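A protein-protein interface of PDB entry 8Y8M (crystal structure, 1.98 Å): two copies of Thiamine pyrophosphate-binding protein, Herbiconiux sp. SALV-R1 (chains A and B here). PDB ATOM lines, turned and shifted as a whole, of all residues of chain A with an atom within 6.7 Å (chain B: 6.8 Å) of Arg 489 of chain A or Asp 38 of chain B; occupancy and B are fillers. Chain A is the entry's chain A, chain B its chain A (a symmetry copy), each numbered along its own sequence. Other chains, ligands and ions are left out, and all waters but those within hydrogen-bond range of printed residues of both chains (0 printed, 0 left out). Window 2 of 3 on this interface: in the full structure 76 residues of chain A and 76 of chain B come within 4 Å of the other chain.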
ATOM      1  N   LEU A 478      13.067  28.433  23.652  1.00  0.00           N
ATOM      2  CA  LEU A 478      11.912  29.303  23.842  1.00  0.00           C
ATOM      3  C   LEU A 478      12.028  30.542  22.964  1.00  0.00           C
ATOM      4  O   LEU A 478      11.056  30.952  22.307  1.00  0.00           O
ATOM      5  CB  LEU A 478      11.763  29.726  25.330  1.00  0.00           C
ATOM      6  CG  LEU A 478      10.447  30.468  25.706  1.00  0.00           C
ATOM      7  CD1 LEU A 478       9.929  30.127  27.089  1.00  0.00           C
ATOM      8  CD2 LEU A 478      10.528  31.982  25.551  1.00  0.00           C
ATOM      9  N   GLN A 481      11.147  30.036  19.275  1.00  0.00           N
ATOM     10  CA  GLN A 481       9.723  30.005  18.967  1.00  0.00           C
ATOM     11  C   GLN A 481       9.112  31.405  19.090  1.00  0.00           C
ATOM     12  O   GLN A 481       8.347  31.833  18.216  1.00  0.00           O
ATOM     13  CB  GLN A 481       8.957  29.020  19.869  1.00  0.00           C
ATOM     14  CG  GLN A 481       9.511  27.594  19.956  1.00  0.00           C
ATOM     15  CD  GLN A 481       8.836  26.820  21.048  1.00  0.00           C
ATOM     16  OE1 GLN A 481       8.754  27.286  22.215  1.00  0.00           O
ATOM     17  NE2 GLN A 481       8.461  25.576  20.742  1.00  0.00           N
ATOM     18  N   GLU A 482       9.440  32.133  20.178  1.00  0.00           N
ATOM     19  CA  GLU A 482       8.726  33.379  20.485  1.00  0.00           C
ATOM     20  C   GLU A 482       9.095  34.501  19.512  1.00  0.00           C
ATOM     21  O   GLU A 482       8.223  35.258  19.072  1.00  0.00           O
ATOM     22  CB  GLU A 482       8.984  33.813  21.933  1.00  0.00           C
ATOM     23  CG  GLU A 482       7.897  34.737  22.445  1.00  0.00           C
ATOM     24  CD  GLU A 482       8.155  35.283  23.837  1.00  0.00           C
ATOM     25  OE1 GLU A 482       8.427  36.500  23.938  1.00  0.00           O
ATOM     26  OE2 GLU A 482       8.098  34.503  24.820  1.00  0.00           O
ATOM     27  N   LEU A 485       8.066  32.956  15.651  1.00  0.00           N
ATOM     28  CA  LEU A 485       6.674  32.582  15.418  1.00  0.00           C
ATOM     29  C   LEU A 485       5.644  33.280  16.293  1.00  0.00           C
ATOM     30  O   LEU A 485       4.478  33.319  15.897  1.00  0.00           O
ATOM     31  CB  LEU A 485       6.485  31.057  15.549  1.00  0.00           C
ATOM     32  CG  LEU A 485       7.543  30.146  14.871  1.00  0.00           C
ATOM     33  CD1 LEU A 485       7.477  28.709  15.368  1.00  0.00           C
ATOM     34  CD2 LEU A 485       7.438  30.194  13.368  1.00  0.00           C
ATOM     35  N   GLY A 486       6.027  33.823  17.456  1.00  0.00           N
ATOM     36  CA  GLY A 486       5.122  34.568  18.313  1.00  0.00           C
ATOM     37  C   GLY A 486       4.938  33.951  19.691  1.00  0.00           C
ATOM     38  O   GLY A 486       5.173  32.756  19.876  1.00  0.00           O
ATOM     39  N   PRO A 487       4.497  34.744  20.686  1.00  0.00           N
ATOM     40  CA  PRO A 487       4.348  34.201  22.056  1.00  0.00           C
ATOM     41  C   PRO A 487       3.394  33.019  22.165  1.00  0.00           C
ATOM     42  O   PRO A 487       3.614  32.133  22.998  1.00  0.00           O
ATOM     43  CB  PRO A 487       3.835  35.411  22.856  1.00  0.00           C
ATOM     44  CG  PRO A 487       4.281  36.573  22.058  1.00  0.00           C
ATOM     45  CD  PRO A 487       4.072  36.150  20.635  1.00  0.00           C
ATOM     46  N   ASP A 488       2.345  32.969  21.351  1.00  0.00           N
ATOM     47  CA  ASP A 488       1.404  31.852  21.387  1.00  0.00           C
ATOM     48  C   ASP A 488       2.007  30.540  20.860  1.00  0.00           C
ATOM     49  O   ASP A 488       1.344  29.497  20.929  1.00  0.00           O
ATOM     50  CB  ASP A 488       0.192  32.205  20.543  1.00  0.00           C
ATOM     51  CG  ASP A 488       0.604  32.794  19.190  1.00  0.00           C
ATOM     52  OD1 ASP A 488       1.565  33.616  19.156  1.00  0.00           O
ATOM     53  OD2 ASP A 488       0.020  32.378  18.155  1.00  0.00           O
ATOM     54  N   ARG A 489       3.231  30.570  20.329  1.00  0.00           N
ATOM     55  CA  ARG A 489       3.856  29.423  19.680  1.00  0.00           C
ATOM     56  C   ARG A 489       4.932  28.807  20.554  1.00  0.00           C
ATOM     57  O   ARG A 489       5.688  27.937  20.086  1.00  0.00           O
ATOM     58  CB  ARG A 489       4.451  29.840  18.330  1.00  0.00           C
ATOM     59  CG  ARG A 489       3.445  30.280  17.259  1.00  0.00           C
ATOM     60  CD  ARG A 489       2.126  29.511  17.245  1.00  0.00           C
ATOM     61  NE  ARG A 489       2.332  28.234  16.574  1.00  0.00           N
ATOM     62  CZ  ARG A 489       1.398  27.341  16.259  1.00  0.00           C
ATOM     63  NH1 ARG A 489       0.106  27.616  16.342  1.00  0.00           N
ATOM     64  NH2 ARG A 489       1.774  26.145  15.815  1.00  0.00           N
ATOM     65  N   VAL A 490       5.054  29.280  21.792  1.00  0.00           N
ATOM     66  CA  VAL A 490       6.018  28.728  22.728  1.00  0.00           C
ATOM     67  C   VAL A 490       5.406  27.450  23.269  1.00  0.00           C
ATOM     68  O   VAL A 490       4.251  27.456  23.689  1.00  0.00           O
ATOM     69  CB  VAL A 490       6.317  29.734  23.858  1.00  0.00           C
ATOM     70  CG1 VAL A 490       6.933  29.028  25.077  1.00  0.00           C
ATOM     71  CG2 VAL A 490       7.199  30.868  23.360  1.00  0.00           C
ATOM     72  N   VAL A 491       6.158  26.345  23.254  1.00  0.00           N
ATOM     73  CA  VAL A 491       5.599  25.091  23.760  1.00  0.00           C
ATOM     74  C   VAL A 491       6.747  24.178  24.161  1.00  0.00           C
ATOM     75  O   VAL A 491       7.813  24.182  23.531  1.00  0.00           O
ATOM     76  CB  VAL A 491       4.670  24.413  22.714  1.00  0.00           C
ATOM     77  CG1 VAL A 491       5.452  23.954  21.471  1.00  0.00           C
ATOM     78  CG2 VAL A 491       3.817  23.284  23.348  1.00  0.00           C
ATOM     79  N   ASN A 493       8.850  24.383  26.608  1.00  0.00           N
ATOM     80  CA  ASN A 493      10.094  25.102  26.931  1.00  0.00           C
ATOM     81  C   ASN A 493      10.102  25.796  28.275  1.00  0.00           C
ATOM     82  O   ASN A 493      11.199  26.097  28.740  1.00  0.00           O
ATOM     83  CB  ASN A 493      10.452  26.156  25.862  1.00  0.00           C
ATOM     84  CG  ASN A 493      11.159  25.530  24.629  1.00  0.00           C
ATOM     85  OD1 ASN A 493      12.093  24.752  24.757  1.00  0.00           O
ATOM     86  ND2 ASN A 493      10.617  25.792  23.468  1.00  0.00           N
ATOM     87  N   GLU B   7       4.368  18.388  10.285  1.00  0.00           N
ATOM     88  CA  GLU B   7       2.948  18.042  10.206  1.00  0.00           C
ATOM     89  C   GLU B   7       2.758  16.608   9.713  1.00  0.00           C
ATOM     90  O   GLU B   7       1.945  15.845  10.273  1.00  0.00           O
ATOM     91  CB  GLU B   7       2.223  19.038   9.287  1.00  0.00           C
ATOM     92  CG  GLU B   7       1.900  20.382   9.992  1.00  0.00           C
ATOM     93  CD  GLU B   7       1.408  21.542   9.069  1.00  0.00           C
ATOM     94  OE1 GLU B   7       1.783  21.643   7.877  1.00  0.00           O
ATOM     95  OE2 GLU B   7       0.667  22.409   9.572  1.00  0.00           O
ATOM     96  N   ASP B  30      11.736  21.483  15.881  1.00  0.00           N
ATOM     97  CA  ASP B  30      10.570  22.251  16.312  1.00  0.00           C
ATOM     98  C   ASP B  30       9.366  22.176  15.378  1.00  0.00           C
ATOM     99  O   ASP B  30       8.236  22.432  15.840  1.00  0.00           O
ATOM    100  CB  ASP B  30      10.895  23.735  16.512  1.00  0.00           C
ATOM    101  CG  ASP B  30       9.847  24.444  17.381  1.00  0.00           C
ATOM    102  OD1 ASP B  30       9.427  23.944  18.463  1.00  0.00           O
ATOM    103  OD2 ASP B  30       9.399  25.502  16.930  1.00  0.00           O
ATOM    104  N   TYR B  33       7.091  19.979  16.946  1.00  0.00           N
ATOM    105  CA  TYR B  33       6.462  20.538  18.150  1.00  0.00           C
ATOM    106  C   TYR B  33       5.368  21.522  17.769  1.00  0.00           C
ATOM    107  O   TYR B  33       4.319  21.587  18.425  1.00  0.00           O
ATOM    108  CB  TYR B  33       7.525  21.199  19.020  1.00  0.00           C
ATOM    109  CG  TYR B  33       8.294  20.202  19.857  1.00  0.00           C
ATOM    110  CD1 TYR B  33       9.249  19.350  19.266  1.00  0.00           C
ATOM    111  CD2 TYR B  33       8.040  20.080  21.227  1.00  0.00           C
ATOM    112  CE1 TYR B  33       9.946  18.416  20.030  1.00  0.00           C
ATOM    113  CE2 TYR B  33       8.730  19.146  21.999  1.00  0.00           C
ATOM    114  CZ  TYR B  33       9.683  18.342  21.419  1.00  0.00           C
ATOM    115  OH  TYR B  33      10.368  17.403  22.187  1.00  0.00           O
ATOM    116  N   GLN B  34       5.599  22.304  16.719  1.00  0.00           N
ATOM    117  CA  GLN B  34       4.579  23.238  16.238  1.00  0.00           C
ATOM    118  C   GLN B  34       3.351  22.507  15.706  1.00  0.00           C
ATOM    119  O   GLN B  34       2.211  22.838  16.063  1.00  0.00           O
ATOM    120  CB  GLN B  34       5.160  24.140  15.152  1.00  0.00           C
ATOM    121  CG  GLN B  34       6.227  25.093  15.649  1.00  0.00           C
ATOM    122  CD  GLN B  34       5.742  25.878  16.879  1.00  0.00           C
ATOM    123  OE1 GLN B  34       4.650  26.473  16.842  1.00  0.00           O
ATOM    124  NE2 GLN B  34       6.568  25.944  17.928  1.00  0.00           N
ATOM    125  N   ALA B  35       3.563  21.509  14.848  1.00  0.00           N
ATOM    126  CA  ALA B  35       2.454  20.692  14.365  1.00  0.00           C
ATOM    127  C   ALA B  35       1.686  20.081  15.520  1.00  0.00           C
ATOM    128  O   ALA B  35       0.451  20.036  15.496  1.00  0.00           O
ATOM    129  CB  ALA B  35       2.964  19.577  13.438  1.00  0.00           C
ATOM    130  N   ALA B  36       2.406  19.580  16.530  1.00  0.00           N
ATOM    131  CA  ALA B  36       1.749  18.933  17.661  1.00  0.00           C
ATOM    132  C   ALA B  36       0.876  19.929  18.420  1.00  0.00           C
ATOM    133  O   ALA B  36      -0.195  19.578  18.929  1.00  0.00           O
ATOM    134  CB  ALA B  36       2.792  18.352  18.616  1.00  0.00           C
ATOM    135  N   LEU B  37       1.330  21.174  18.517  1.00  0.00           N
ATOM    136  CA  LEU B  37       0.526  22.181  19.203  1.00  0.00           C
ATOM    137  C   LEU B  37      -0.770  22.443  18.437  1.00  0.00           C
ATOM    138  O   LEU B  37      -1.846  22.471  19.041  1.00  0.00           O
ATOM    139  CB  LEU B  37       1.339  23.467  19.404  1.00  0.00           C
ATOM    140  CG  LEU B  37       0.637  24.716  19.976  1.00  0.00           C
ATOM    141  CD1 LEU B  37       0.238  24.435  21.421  1.00  0.00           C
ATOM    142  CD2 LEU B  37       1.568  25.937  19.943  1.00  0.00           C
ATOM    143  N   ASP B  38      -0.691  22.574  17.101  1.00  0.00           N
ATOM    144  CA  ASP B  38      -1.886  22.747  16.260  1.00  0.00           C
ATOM    145  C   ASP B  38      -2.883  21.600  16.327  1.00  0.00           C
ATOM    146  O   ASP B  38      -4.068  21.820  16.076  1.00  0.00           O
ATOM    147  CB  ASP B  38      -1.537  22.972  14.782  1.00  0.00           C
ATOM    148  CG  ASP B  38      -0.859  24.282  14.538  1.00  0.00           C
ATOM    149  OD1 ASP B  38      -1.144  25.224  15.279  1.00  0.00           O
ATOM    150  OD2 ASP B  38      -0.081  24.409  13.587  1.00  0.00           O
ATOM    151  N   ARG B  39      -2.443  20.382  16.582  1.00  0.00           N
ATOM    152  CA  ARG B  39      -3.299  19.201  16.561  1.00  0.00           C
ATOM    153  C   ARG B  39      -3.574  18.671  17.938  1.00  0.00           C
ATOM    154  O   ARG B  39      -4.070  17.546  18.053  1.00  0.00           O
ATOM    155  CB  ARG B  39      -2.621  18.096  15.748  1.00  0.00           C
ATOM    156  CG  ARG B  39      -1.839  18.633  14.593  1.00  0.00           C
ATOM    157  CD  ARG B  39      -2.259  18.333  13.176  1.00  0.00           C
ATOM    158  NE  ARG B  39      -2.998  17.077  13.071  1.00  0.00           N
ATOM    159  CZ  ARG B  39      -3.771  16.744  12.048  1.00  0.00           C
ATOM    160  NH1 ARG B  39      -3.825  17.493  10.959  1.00  0.00           N
ATOM    161  NH2 ARG B  39      -4.477  15.613  12.106  1.00  0.00           N
ATOM    162  N   SER B  40      -3.191  19.413  18.979  1.00  0.00           N
ATOM    163  CA  SER B  40      -3.324  18.979  20.360  1.00  0.00           C
ATOM    164  C   SER B  40      -2.748  17.578  20.564  1.00  0.00           C
ATOM    165  O   SER B  40      -3.356  16.696  21.180  1.00  0.00           O
ATOM    166  CB  SER B  40      -4.783  19.068  20.818  1.00  0.00           C
ATOM    167  OG  SER B  40      -5.213  20.413  20.733  1.00  0.00           O
ATOM    168  N   PHE B  41      -1.533  17.382  20.056  1.00  0.00           N
ATOM    169  CA  PHE B  41      -0.812  16.141  20.287  1.00  0.00           C
ATOM    170  C   PHE B  41       0.113  16.360  21.479  1.00  0.00           C
ATOM    171  O   PHE B  41       0.877  17.319  21.488  1.00  0.00           O
ATOM    172  CB  PHE B  41      -0.009  15.750  19.036  1.00  0.00           C
ATOM    173  CG  PHE B  41       0.709  14.443  19.171  1.00  0.00           C
ATOM    174  CD1 PHE B  41       1.979  14.416  19.726  1.00  0.00           C
ATOM    175  CD2 PHE B  41       0.188  13.265  18.656  1.00  0.00           C
ATOM    176  CE1 PHE B  41       2.678  13.231  19.883  1.00  0.00           C
ATOM    177  CE2 PHE B  41       0.885  12.085  18.777  1.00  0.00           C
ATOM    178  CZ  PHE B  41       2.141  12.056  19.387  1.00  0.00           C
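Among the printed residues, merely in contact across the chains: Leu 485 of chain A with Gln 34 of chain B (3.6 Å), Asp 488 of chain A with Leu 37 of chain B (3.7 Å) and Arg 489 of chain A with Leu 37 of chain B (3.9 Å).
Of the printed residues of chain B, Arg 489 of chain A touches Gln 34, Leu 37 and Asp 38. Asp 38 of chain B touches just one residue of chain A: Arg 489. Of the printed residues of chain B, Leu 485 of chain A touches Gln 34 (3.6 Å). Of the printed residues of chain B, Asp 488 of chain A touches Leu 37. Ser 40 of chain B touches none of the printed residues of chain A. Asn 493 of chain A touches none of the printed residues of chain B. The nearest residue of chain B that does not touch Arg 489 of chain A is Ala 35 of chain B (5.1 Å).
The side-chain amide nitrogen of Gln 34 of chain B lies within hydrogen-bond range of the side-chain carboxylate of Asp 30 of chain B. The side-chain amide oxygen of Gln 481 of chain A lies within hydrogen-bond range of the side-chain amide nitrogen of Asn 493 of chain A (2.7 Å). O of Gln 481 of chain A is in hydrogen-bond range of N of Gly 486 of chain A, at 3.1 Å. The backbone NH of Val 491 of chain A is in hydrogen-bond range of the side-chain amide oxygen of Gln 481 of chain A (3.0 Å).
NE2 of Gln 481 of chain A lies close to NE2 of Gln 34 of chain B, at 3.4 Å. NE2 of Gln 481 of chain A is in hydrogen-bond range of OD1 of Asp 30 of chain B, at 3.0 Å. The guanidinium group of Arg 489 of chain A lies within salt-bridge range of the side-chain carboxylate of Asp 38 of chain B, at 2.9 Å. NE of Arg 489 of chain A lies within hydrogen-bond range of OE1 of Gln 34 of chain B.
Of the 11 printed residues of chain B, 4 touch a printed residue of chain A. Printed residues of chain B that touch a printed residue of chain A: Asp 30, Gln 34, Leu 37 and Asp 38. Hydrophobic or aromatic side chains of chain A that line the printed part of chain B: Leu 485. Among the printed residues, 7 pairs touch across the chains.
No position is printed for both chains.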
